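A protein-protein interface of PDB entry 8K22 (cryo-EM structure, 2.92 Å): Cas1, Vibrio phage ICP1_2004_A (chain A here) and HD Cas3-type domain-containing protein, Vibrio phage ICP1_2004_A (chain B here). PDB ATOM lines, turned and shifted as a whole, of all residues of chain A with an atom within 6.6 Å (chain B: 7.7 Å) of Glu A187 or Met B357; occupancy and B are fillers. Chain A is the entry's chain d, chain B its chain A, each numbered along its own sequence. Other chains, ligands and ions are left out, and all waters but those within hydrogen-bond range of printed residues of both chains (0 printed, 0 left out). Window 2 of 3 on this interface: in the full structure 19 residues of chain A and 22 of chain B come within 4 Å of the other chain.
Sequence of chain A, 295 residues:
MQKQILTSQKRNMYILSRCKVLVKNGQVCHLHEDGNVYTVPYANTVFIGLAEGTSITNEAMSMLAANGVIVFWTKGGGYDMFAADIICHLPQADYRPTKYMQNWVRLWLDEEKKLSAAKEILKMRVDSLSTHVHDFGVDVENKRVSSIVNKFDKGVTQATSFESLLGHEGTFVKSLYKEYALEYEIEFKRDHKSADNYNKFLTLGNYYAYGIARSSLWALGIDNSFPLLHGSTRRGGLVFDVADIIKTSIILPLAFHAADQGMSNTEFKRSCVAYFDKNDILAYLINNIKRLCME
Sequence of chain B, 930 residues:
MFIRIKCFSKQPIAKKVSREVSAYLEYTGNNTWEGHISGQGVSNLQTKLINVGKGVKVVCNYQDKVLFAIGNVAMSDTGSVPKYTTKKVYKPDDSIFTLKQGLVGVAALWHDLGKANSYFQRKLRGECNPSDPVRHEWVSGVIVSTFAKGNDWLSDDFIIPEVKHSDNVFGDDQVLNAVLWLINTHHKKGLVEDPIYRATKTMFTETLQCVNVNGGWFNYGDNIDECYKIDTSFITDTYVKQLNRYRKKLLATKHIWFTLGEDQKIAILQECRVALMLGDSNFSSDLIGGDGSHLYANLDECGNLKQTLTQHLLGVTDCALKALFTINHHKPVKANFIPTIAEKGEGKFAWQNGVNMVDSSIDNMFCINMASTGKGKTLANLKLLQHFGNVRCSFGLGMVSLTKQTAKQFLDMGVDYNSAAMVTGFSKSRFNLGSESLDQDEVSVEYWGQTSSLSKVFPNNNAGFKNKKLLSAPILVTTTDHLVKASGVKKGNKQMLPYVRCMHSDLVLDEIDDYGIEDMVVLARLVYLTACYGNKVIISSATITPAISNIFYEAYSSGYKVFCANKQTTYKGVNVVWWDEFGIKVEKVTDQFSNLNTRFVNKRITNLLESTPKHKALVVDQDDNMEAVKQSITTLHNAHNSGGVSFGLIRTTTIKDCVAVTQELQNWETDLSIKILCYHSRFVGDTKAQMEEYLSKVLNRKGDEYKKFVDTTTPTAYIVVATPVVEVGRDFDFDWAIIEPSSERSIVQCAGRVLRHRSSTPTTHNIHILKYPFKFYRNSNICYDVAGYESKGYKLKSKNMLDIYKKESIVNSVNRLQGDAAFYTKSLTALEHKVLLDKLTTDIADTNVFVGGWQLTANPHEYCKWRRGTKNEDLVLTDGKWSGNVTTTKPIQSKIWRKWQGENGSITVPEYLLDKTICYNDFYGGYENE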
ATOM      1  N   LYS A 178       9.634  -1.780  -1.748  1.00  0.00           N
ATOM      2  CA  LYS A 178       9.550  -2.561  -2.980  1.00  0.00           C
ATOM      3  C   LYS A 178       8.142  -2.730  -3.498  1.00  0.00           C
ATOM      4  O   LYS A 178       7.940  -2.909  -4.688  1.00  0.00           O
ATOM      5  CB  LYS A 178      10.182  -3.934  -2.812  1.00  0.00           C
ATOM      6  CG  LYS A 178      11.291  -4.229  -3.807  1.00  0.00           C
ATOM      7  CD  LYS A 178      11.885  -2.954  -4.384  1.00  0.00           C
ATOM      8  CE  LYS A 178      12.361  -3.166  -5.813  1.00  0.00           C
ATOM      9  NZ  LYS A 178      11.237  -3.489  -6.733  1.00  0.00           N
ATOM     10  N   ALA A 181       7.509   0.319  -5.252  1.00  0.00           N
ATOM     11  CA  ALA A 181       8.240   0.280  -6.493  1.00  0.00           C
ATOM     12  C   ALA A 181       7.452  -0.494  -7.509  1.00  0.00           C
ATOM     13  O   ALA A 181       7.423  -0.134  -8.673  1.00  0.00           O
ATOM     14  CB  ALA A 181       9.582  -0.361  -6.289  1.00  0.00           C
ATOM     15  N   TYR A 184       4.474   1.612  -8.803  1.00  0.00           N
ATOM     16  CA  TYR A 184       4.859   2.692  -9.678  1.00  0.00           C
ATOM     17  C   TYR A 184       5.743   2.140 -10.764  1.00  0.00           C
ATOM     18  O   TYR A 184       6.407   2.901 -11.458  1.00  0.00           O
ATOM     19  CB  TYR A 184       5.561   3.776  -8.881  1.00  0.00           C
ATOM     20  CG  TYR A 184       4.631   4.633  -8.052  1.00  0.00           C
ATOM     21  CD1 TYR A 184       4.192   4.224  -6.800  1.00  0.00           C
ATOM     22  CD2 TYR A 184       4.200   5.854  -8.519  1.00  0.00           C
ATOM     23  CE1 TYR A 184       3.349   5.012  -6.044  1.00  0.00           C
ATOM     24  CE2 TYR A 184       3.355   6.647  -7.775  1.00  0.00           C
ATOM     25  CZ  TYR A 184       2.936   6.226  -6.538  1.00  0.00           C
ATOM     26  OH  TYR A 184       2.100   7.032  -5.804  1.00  0.00           O
ATOM     27  N   GLU A 185       5.778   0.823 -10.897  1.00  0.00           N
ATOM     28  CA  GLU A 185       6.540   0.170 -11.952  1.00  0.00           C
ATOM     29  C   GLU A 185       7.954   0.629 -12.136  1.00  0.00           C
ATOM     30  O   GLU A 185       8.389   0.833 -13.263  1.00  0.00           O
ATOM     31  CB  GLU A 185       5.793   0.252 -13.278  1.00  0.00           C
ATOM     32  CG  GLU A 185       4.739  -0.825 -13.449  1.00  0.00           C
ATOM     33  CD  GLU A 185       3.382  -0.392 -12.936  1.00  0.00           C
ATOM     34  OE1 GLU A 185       3.013   0.780 -13.154  1.00  0.00           O
ATOM     35  OE2 GLU A 185       2.688  -1.222 -12.310  1.00  0.00           O
ATOM     36  N   ILE A 186       8.690   0.782 -11.049  1.00  0.00           N
ATOM     37  CA  ILE A 186      10.091   1.119 -11.188  1.00  0.00           C
ATOM     38  C   ILE A 186      10.944   0.179 -10.385  1.00  0.00           C
ATOM     39  O   ILE A 186      10.442  -0.587  -9.576  1.00  0.00           O
ATOM     40  CB  ILE A 186      10.403   2.554 -10.740  1.00  0.00           C
ATOM     41  CG1 ILE A 186       9.791   2.844  -9.375  1.00  0.00           C
ATOM     42  CG2 ILE A 186       9.951   3.569 -11.780  1.00  0.00           C
ATOM     43  CD1 ILE A 186      10.826   3.297  -8.377  1.00  0.00           C
ATOM     44  N   GLU A 187      12.242   0.219 -10.620  1.00  0.00           N
ATOM     45  CA  GLU A 187      13.146  -0.589  -9.833  1.00  0.00           C
ATOM     46  C   GLU A 187      13.644   0.345  -8.772  1.00  0.00           C
ATOM     47  O   GLU A 187      14.129   1.426  -9.080  1.00  0.00           O
ATOM     48  CB  GLU A 187      14.317  -1.053 -10.682  1.00  0.00           C
ATOM     49  CG  GLU A 187      14.338  -0.482 -12.091  1.00  0.00           C
ATOM     50  CD  GLU A 187      15.064   0.847 -12.175  1.00  0.00           C
ATOM     51  OE1 GLU A 187      14.396   1.873 -12.426  1.00  0.00           O
ATOM     52  OE2 GLU A 187      16.297   0.866 -11.981  1.00  0.00           O
ATOM     53  N   PHE A 188      13.519  -0.030  -7.513  1.00  0.00           N
ATOM     54  CA  PHE A 188      13.912   0.913  -6.492  1.00  0.00           C
ATOM     55  C   PHE A 188      14.943   0.448  -5.502  1.00  0.00           C
ATOM     56  O   PHE A 188      14.820  -0.627  -4.929  1.00  0.00           O
ATOM     57  CB  PHE A 188      12.713   1.444  -5.727  1.00  0.00           C
ATOM     58  CG  PHE A 188      13.043   2.637  -4.917  1.00  0.00           C
ATOM     59  CD1 PHE A 188      13.587   3.747  -5.527  1.00  0.00           C
ATOM     60  CD2 PHE A 188      12.882   2.631  -3.552  1.00  0.00           C
ATOM     61  CE1 PHE A 188      13.937   4.846  -4.794  1.00  0.00           C
ATOM     62  CE2 PHE A 188      13.229   3.731  -2.813  1.00  0.00           C
ATOM     63  CZ  PHE A 188      13.756   4.839  -3.436  1.00  0.00           C
ATOM     64  N   LYS A 189      15.963   1.268  -5.289  1.00  0.00           N
ATOM     65  CA  LYS A 189      16.966   0.960  -4.292  1.00  0.00           C
ATOM     66  C   LYS A 189      17.181   2.254  -3.548  1.00  0.00           C
ATOM     67  O   LYS A 189      17.401   3.289  -4.163  1.00  0.00           O
ATOM     68  CB  LYS A 189      18.266   0.504  -4.943  1.00  0.00           C
ATOM     69  CG  LYS A 189      18.423   0.906  -6.402  1.00  0.00           C
ATOM     70  CD  LYS A 189      18.470  -0.313  -7.311  1.00  0.00           C
ATOM     71  CE  LYS A 189      17.591  -0.117  -8.533  1.00  0.00           C
ATOM     72  NZ  LYS A 189      17.131   1.294  -8.655  1.00  0.00           N
ATOM     73  N   ALA A 195      20.879  10.085  -8.238  1.00  0.00           N
ATOM     74  CA  ALA A 195      20.281  11.127  -9.053  1.00  0.00           C
ATOM     75  C   ALA A 195      18.834  10.834  -9.426  1.00  0.00           C
ATOM     76  O   ALA A 195      18.175  11.698 -10.015  1.00  0.00           O
ATOM     77  CB  ALA A 195      21.102  11.341 -10.329  1.00  0.00           C
ATOM     78  N   ASP A 196      18.329   9.651  -9.100  1.00  0.00           N
ATOM     79  CA  ASP A 196      16.960   9.287  -9.427  1.00  0.00           C
ATOM     80  C   ASP A 196      15.968  10.007  -8.521  1.00  0.00           C
ATOM     81  O   ASP A 196      16.201  10.136  -7.312  1.00  0.00           O
ATOM     82  CB  ASP A 196      16.804   7.771  -9.319  1.00  0.00           C
ATOM     83  CG  ASP A 196      15.378   7.344  -9.103  1.00  0.00           C
ATOM     84  OD1 ASP A 196      14.578   7.387 -10.061  1.00  0.00           O
ATOM     85  OD2 ASP A 196      15.064   6.949  -7.969  1.00  0.00           O
ATOM     86  N   ASN A 197      14.852  10.477  -9.110  1.00  0.00           N
ATOM     87  CA  ASN A 197      13.916  11.344  -8.388  1.00  0.00           C
ATOM     88  C   ASN A 197      13.187  10.660  -7.250  1.00  0.00           C
ATOM     89  O   ASN A 197      12.893  11.330  -6.253  1.00  0.00           O
ATOM     90  CB  ASN A 197      12.909  11.942  -9.385  1.00  0.00           C
ATOM     91  CG  ASN A 197      13.573  12.502 -10.611  1.00  0.00           C
ATOM     92  OD1 ASN A 197      14.066  11.758 -11.446  1.00  0.00           O
ATOM     93  ND2 ASN A 197      13.562  13.826 -10.749  1.00  0.00           N
ATOM     94  N   TYR A 198      12.982   9.344  -7.336  1.00  0.00           N
ATOM     95  CA  TYR A 198      12.390   8.600  -6.224  1.00  0.00           C
ATOM     96  C   TYR A 198      13.312   8.586  -5.009  1.00  0.00           C
ATOM     97  O   TYR A 198      12.845   8.398  -3.882  1.00  0.00           O
ATOM     98  CB  TYR A 198      12.084   7.167  -6.665  1.00  0.00           C
ATOM     99  CG  TYR A 198      11.038   7.054  -7.753  1.00  0.00           C
ATOM    100  CD1 TYR A 198      11.402   7.085  -9.099  1.00  0.00           C
ATOM    101  CD2 TYR A 198       9.697   6.890  -7.445  1.00  0.00           C
ATOM    102  CE1 TYR A 198      10.456   6.973 -10.107  1.00  0.00           C
ATOM    103  CE2 TYR A 198       8.742   6.780  -8.446  1.00  0.00           C
ATOM    104  CZ  TYR A 198       9.129   6.821  -9.775  1.00  0.00           C
ATOM    105  OH  TYR A 198       8.188   6.709 -10.777  1.00  0.00           O
ATOM    106  N   LYS A 200      15.968  11.244  -4.280  1.00  0.00           N
ATOM    107  CA  LYS A 200      16.179  12.532  -3.626  1.00  0.00           C
ATOM    108  C   LYS A 200      14.871  13.158  -3.169  1.00  0.00           C
ATOM    109  O   LYS A 200      14.874  13.972  -2.235  1.00  0.00           O
ATOM    110  CB  LYS A 200      16.996  13.523  -4.465  1.00  0.00           C
ATOM    111  CG  LYS A 200      16.236  14.413  -5.403  1.00  0.00           C
ATOM    112  CD  LYS A 200      17.042  14.514  -6.677  1.00  0.00           C
ATOM    113  CE  LYS A 200      16.722  13.413  -7.604  1.00  0.00           C
ATOM    114  NZ  LYS A 200      17.170  13.677  -8.984  1.00  0.00           N
ATOM    115  N   ALA A 259       7.665  11.878  -7.686  1.00  0.00           N
ATOM    116  CA  ALA A 259       8.627  11.411  -8.672  1.00  0.00           C
ATOM    117  C   ALA A 259       7.965  10.732  -9.858  1.00  0.00           C
ATOM    118  O   ALA A 259       8.636  10.491 -10.866  1.00  0.00           O
ATOM    119  CB  ALA A 259       9.626  10.450  -8.024  1.00  0.00           C
ATOM    120  N   TRP B 351       6.976   5.639 -22.848  1.00  0.00           N
ATOM    121  CA  TRP B 351       8.393   5.780 -22.539  1.00  0.00           C
ATOM    122  C   TRP B 351       8.785   7.225 -22.267  1.00  0.00           C
ATOM    123  O   TRP B 351       9.838   7.466 -21.665  1.00  0.00           O
ATOM    124  CB  TRP B 351       9.232   5.224 -23.684  1.00  0.00           C
ATOM    125  CG  TRP B 351       9.033   5.950 -24.971  1.00  0.00           C
ATOM    126  CD1 TRP B 351       8.033   5.755 -25.872  1.00  0.00           C
ATOM    127  CD2 TRP B 351       9.867   6.975 -25.515  1.00  0.00           C
ATOM    128  NE1 TRP B 351       8.183   6.603 -26.938  1.00  0.00           N
ATOM    129  CE2 TRP B 351       9.305   7.362 -26.744  1.00  0.00           C
ATOM    130  CE3 TRP B 351      11.034   7.607 -25.080  1.00  0.00           C
ATOM    131  CZ2 TRP B 351       9.867   8.350 -27.541  1.00  0.00           C
ATOM    132  CZ3 TRP B 351      11.591   8.586 -25.874  1.00  0.00           C
ATOM    133  CH2 TRP B 351      11.008   8.946 -27.092  1.00  0.00           C
ATOM    134  N   GLN B 352       7.943   8.190 -22.654  1.00  0.00           N
ATOM    135  CA  GLN B 352       8.235   9.602 -22.438  1.00  0.00           C
ATOM    136  C   GLN B 352       8.173  10.009 -20.971  1.00  0.00           C
ATOM    137  O   GLN B 352       8.554  11.138 -20.647  1.00  0.00           O
ATOM    138  CB  GLN B 352       7.282  10.466 -23.260  1.00  0.00           C
ATOM    139  CG  GLN B 352       7.486  10.333 -24.757  1.00  0.00           C
ATOM    140  CD  GLN B 352       6.679  11.339 -25.545  1.00  0.00           C
ATOM    141  OE1 GLN B 352       5.908  12.112 -24.979  1.00  0.00           O
ATOM    142  NE2 GLN B 352       6.852  11.336 -26.861  1.00  0.00           N
ATOM    143  N   ASN B 353       7.713   9.127 -20.084  1.00  0.00           N
ATOM    144  CA  ASN B 353       7.845   9.297 -18.643  1.00  0.00           C
ATOM    145  C   ASN B 353       9.259   9.015 -18.134  1.00  0.00           C
ATOM    146  O   ASN B 353       9.493   9.081 -16.920  1.00  0.00           O
ATOM    147  CB  ASN B 353       6.844   8.396 -17.919  1.00  0.00           C
ATOM    148  CG  ASN B 353       5.451   8.495 -18.501  1.00  0.00           C
ATOM    149  OD1 ASN B 353       5.035   9.553 -18.971  1.00  0.00           O
ATOM    150  ND2 ASN B 353       4.720   7.387 -18.474  1.00  0.00           N
ATOM    151  N   GLY B 354      10.209   8.713 -19.024  1.00  0.00           N
ATOM    152  CA  GLY B 354      11.610   8.640 -18.645  1.00  0.00           C
ATOM    153  C   GLY B 354      12.184   9.936 -18.112  1.00  0.00           C
ATOM    154  O   GLY B 354      13.182   9.894 -17.383  1.00  0.00           O
ATOM    155  N   VAL B 355      11.564  11.077 -18.432  1.00  0.00           N
ATOM    156  CA  VAL B 355      11.938  12.352 -17.836  1.00  0.00           C
ATOM    157  C   VAL B 355      11.690  12.379 -16.335  1.00  0.00           C
ATOM    158  O   VAL B 355      12.311  13.178 -15.627  1.00  0.00           O
ATOM    159  CB  VAL B 355      11.189  13.505 -18.524  1.00  0.00           C
ATOM    160  CG1 VAL B 355      11.557  13.548 -19.970  1.00  0.00           C
ATOM    161  CG2 VAL B 355       9.685  13.343 -18.377  1.00  0.00           C
ATOM    162  N   ASN B 356      10.810  11.514 -15.818  1.00  0.00           N
ATOM    163  CA  ASN B 356      10.650  11.402 -14.373  1.00  0.00           C
ATOM    164  C   ASN B 356      11.765  10.585 -13.727  1.00  0.00           C
ATOM    165  O   ASN B 356      11.752  10.388 -12.507  1.00  0.00           O
ATOM    166  CB  ASN B 356       9.277  10.824 -14.044  1.00  0.00           C
ATOM    167  CG  ASN B 356       8.166  11.458 -14.858  1.00  0.00           C
ATOM    168  OD1 ASN B 356       8.153  11.400 -16.081  1.00  0.00           O
ATOM    169  ND2 ASN B 356       7.209  12.060 -14.167  1.00  0.00           N
ATOM    170  N   MET B 357      12.709  10.073 -14.516  1.00  0.00           N
ATOM    171  CA  MET B 357      13.922   9.487 -13.965  1.00  0.00           C
ATOM    172  C   MET B 357      15.132  10.411 -14.059  1.00  0.00           C
ATOM    173  O   MET B 357      16.210  10.037 -13.585  1.00  0.00           O
ATOM    174  CB  MET B 357      14.228   8.169 -14.671  1.00  0.00           C
ATOM    175  CG  MET B 357      13.043   7.222 -14.774  1.00  0.00           C
ATOM    176  SD  MET B 357      12.828   6.204 -13.304  1.00  0.00           S
ATOM    177  CE  MET B 357      14.526   5.753 -12.963  1.00  0.00           C
ATOM    178  N   VAL B 358      14.988  11.595 -14.651  1.00  0.00           N
ATOM    179  CA  VAL B 358      16.095  12.538 -14.784  1.00  0.00           C
ATOM    180  C   VAL B 358      15.981  13.608 -13.708  1.00  0.00           C
ATOM    181  O   VAL B 358      14.875  14.013 -13.331  1.00  0.00           O
ATOM    182  CB  VAL B 358      16.106  13.164 -16.191  1.00  0.00           C
ATOM    183  CG1 VAL B 358      17.481  13.727 -16.521  1.00  0.00           C
ATOM    184  CG2 VAL B 358      15.698  12.139 -17.229  1.00  0.00           C
ATOM    185  N   ASP B 359      17.126  14.064 -13.199  1.00  0.00           N
ATOM    186  CA  ASP B 359      17.129  15.105 -12.181  1.00  0.00           C
ATOM    187  C   ASP B 359      16.711  16.431 -12.801  1.00  0.00           C
ATOM    188  O   ASP B 359      17.151  16.778 -13.899  1.00  0.00           O
ATOM    189  CB  ASP B 359      18.514  15.238 -11.549  1.00  0.00           C
ATOM    190  CG  ASP B 359      18.582  16.370 -10.536  1.00  0.00           C
ATOM    191  OD1 ASP B 359      17.588  16.576  -9.808  1.00  0.00           O
ATOM    192  OD2 ASP B 359      19.621  17.051 -10.452  1.00  0.00           O
ATOM    193  N   SER B 360      15.857  17.172 -12.099  1.00  0.00           N
ATOM    194  CA  SER B 360      15.371  18.441 -12.616  1.00  0.00           C
ATOM    195  C   SER B 360      16.286  19.610 -12.283  1.00  0.00           C
ATOM    196  O   SER B 360      16.027  20.725 -12.748  1.00  0.00           O
ATOM    197  CB  SER B 360      13.970  18.725 -12.076  1.00  0.00           C
ATOM    198  OG  SER B 360      13.984  18.792 -10.662  1.00  0.00           O
ATOM    199  N   LEU B 384      11.792  16.602 -22.116  1.00  0.00           N
ATOM    200  CA  LEU B 384      13.051  16.602 -21.379  1.00  0.00           C
ATOM    201  C   LEU B 384      13.523  18.017 -21.089  1.00  0.00           C
ATOM    202  O   LEU B 384      14.070  18.282 -20.013  1.00  0.00           O
ATOM    203  CB  LEU B 384      14.112  15.825 -22.154  1.00  0.00           C
ATOM    204  CG  LEU B 384      15.411  15.528 -21.407  1.00  0.00           C
ATOM    205  CD1 LEU B 384      15.136  14.984 -20.015  1.00  0.00           C
ATOM    206  CD2 LEU B 384      16.246  14.550 -22.198  1.00  0.00           C
ATOM    207  N   HIS B 387      11.312  19.344 -18.290  1.00  0.00           N
ATOM    208  CA  HIS B 387      11.507  18.719 -16.987  1.00  0.00           C
ATOM    209  C   HIS B 387      12.437  19.534 -16.093  1.00  0.00           C
ATOM    210  O   HIS B 387      12.273  19.530 -14.868  1.00  0.00           O
ATOM    211  CB  HIS B 387      12.039  17.297 -17.156  1.00  0.00           C
ATOM    212  CG  HIS B 387      12.305  16.601 -15.861  1.00  0.00           C
ATOM    213  ND1 HIS B 387      11.309  16.316 -14.953  1.00  0.00           N
ATOM    214  CD2 HIS B 387      13.455  16.141 -15.314  1.00  0.00           C
ATOM    215  CE1 HIS B 387      11.833  15.711 -13.902  1.00  0.00           C
ATOM    216  NE2 HIS B 387      13.133  15.589 -14.098  1.00  0.00           N
ATOM    217  N   VAL B 577      22.258  11.365 -20.515  1.00  0.00           N
ATOM    218  CA  VAL B 577      20.938  10.755 -20.447  1.00  0.00           C
ATOM    219  C   VAL B 577      20.757   9.935 -21.718  1.00  0.00           C
ATOM    220  O   VAL B 577      20.378  10.464 -22.770  1.00  0.00           O
ATOM    221  CB  VAL B 577      19.832  11.803 -20.284  1.00  0.00           C
ATOM    222  CG1 VAL B 577      18.483  11.136 -20.166  1.00  0.00           C
ATOM    223  CG2 VAL B 577      20.095  12.646 -19.057  1.00  0.00           C
ATOM    224  N   GLY B 583      13.525   2.574 -22.512  1.00  0.00           N
ATOM    225  CA  GLY B 583      13.986   2.996 -21.208  1.00  0.00           C
ATOM    226  C   GLY B 583      14.837   4.247 -21.284  1.00  0.00           C
ATOM    227  O   GLY B 583      14.982   4.877 -22.336  1.00  0.00           O
ATOM    228  N   ILE B 584      15.382   4.596 -20.119  1.00  0.00           N
ATOM    229  CA  ILE B 584      16.243   5.756 -19.941  1.00  0.00           C
ATOM    230  C   ILE B 584      17.342   5.375 -18.954  1.00  0.00           C
ATOM    231  O   ILE B 584      17.229   4.396 -18.212  1.00  0.00           O
ATOM    232  CB  ILE B 584      15.443   6.992 -19.458  1.00  0.00           C
ATOM    233  CG1 ILE B 584      16.082   8.298 -19.932  1.00  0.00           C
ATOM    234  CG2 ILE B 584      15.268   6.988 -17.962  1.00  0.00           C
ATOM    235  CD1 ILE B 584      15.137   9.460 -20.001  1.00  0.00           C
ATOM    236  N   LYS B 585      18.430   6.140 -18.981  1.00  0.00           N
ATOM    237  CA  LYS B 585      19.541   5.929 -18.058  1.00  0.00           C
ATOM    238  C   LYS B 585      20.296   7.240 -17.916  1.00  0.00           C
ATOM    239  O   LYS B 585      20.789   7.783 -18.908  1.00  0.00           O
ATOM    240  CB  LYS B 585      20.463   4.810 -18.553  1.00  0.00           C
ATOM    241  CG  LYS B 585      21.875   4.848 -18.001  1.00  0.00           C
ATOM    242  CD  LYS B 585      22.721   3.733 -18.589  1.00  0.00           C
ATOM    243  CE  LYS B 585      22.259   2.376 -18.086  1.00  0.00           C
ATOM    244  NZ  LYS B 585      22.058   2.372 -16.610  1.00  0.00           N
ATOM    245  N   VAL B 586      20.375   7.759 -16.694  1.00  0.00           N
ATOM    246  CA  VAL B 586      21.042   9.024 -16.415  1.00  0.00           C
ATOM    247  C   VAL B 586      22.260   8.735 -15.554  1.00  0.00           C
ATOM    248  O   VAL B 586      22.124   8.251 -14.423  1.00  0.00           O
ATOM    249  CB  VAL B 586      20.110  10.021 -15.713  1.00  0.00           C
ATOM    250  CG1 VAL B 586      20.788  11.372 -15.577  1.00  0.00           C
ATOM    251  CG2 VAL B 586      18.803  10.148 -16.471  1.00  0.00           C
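The side-chain amide oxygen of Asn A197 sits close to the backbone carbonyl oxygen of Asn B356 (2.9 Å). The side-chain amino group (NZ) of Lys A200 lies within salt-bridge range of the side-chain carboxylate (OD1) of Asp B359 (3.0 Å). O of Val B358 is in hydrogen-bond range of ND2 of Asn A197 (2.9 Å). The backbone carbonyl oxygen of Met B357 sits close to the side-chain amide oxygen of Asn A197.
The backbone carbonyl oxygen (O) of Val B358 lies within hydrogen-bond range of a ring nitrogen (NE2) of His B387, at 2.5 Å. NZ of Lys A189 is in salt-bridge range of OE2 of Glu A187. N of Tyr A198 sits at hydrogen-bond distance from OD2 of Asp A196, at 3.2 Å. O of Asn B353 sits close to OD1 of Asn B356 (2.8 Å). The backbone carbonyl oxygen of Val B355 sits at hydrogen-bond distance from a ring nitrogen (NE2) of His B387. The backbone carbonyl oxygen (O) of Ala A195 lies within hydrogen-bond range of the side-chain amino group (NZ) of Lys A200 (2.4 Å).
Met B357 touches Glu A187. O of Ala A195 touches CB of Asp B359, 3.9 Å away. Asp A196 touches Met B357. His B387 touches Asn A197. Asn B356 touches Ala A259.
Of the printed residues of chain B, Asp A196 touches Met B357 (3.3 Å). Printed residues of chain B within 4 Å of Lys A200: Asp B359 (3.0 Å). Of the printed residues of chain B, Ala A259 touches Asn B356 (3.3 Å). Printed residues of chain A within 4 Å of Asn B356: Asn A197 (2.9 Å) and Ala A259 (3.3 Å). Met B357 touches just these residues of chain A: Glu A187, Asp A196 and Asn A197. The nearest residue of chain A that does not touch Met B357 is Tyr A198 (4.1 Å). The nearest printed residue of chain A that does not touch Asn B356 is Tyr A198 (4.4 Å).
Of the 17 printed residues of chain B, 5 touch a printed residue of chain A. Hydrophobic or aromatic side chains of chain B that line the printed part of chain A: Met B357 and His B387. Of the 14 printed residues of chain A, 6 touch a printed residue of chain B. Among the printed residues, Asp or Glu carboxylates within 4 Å of a Lys or Arg side-chain nitrogen of the other chain: Lys A200 with Asp B359 (3.0 Å).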
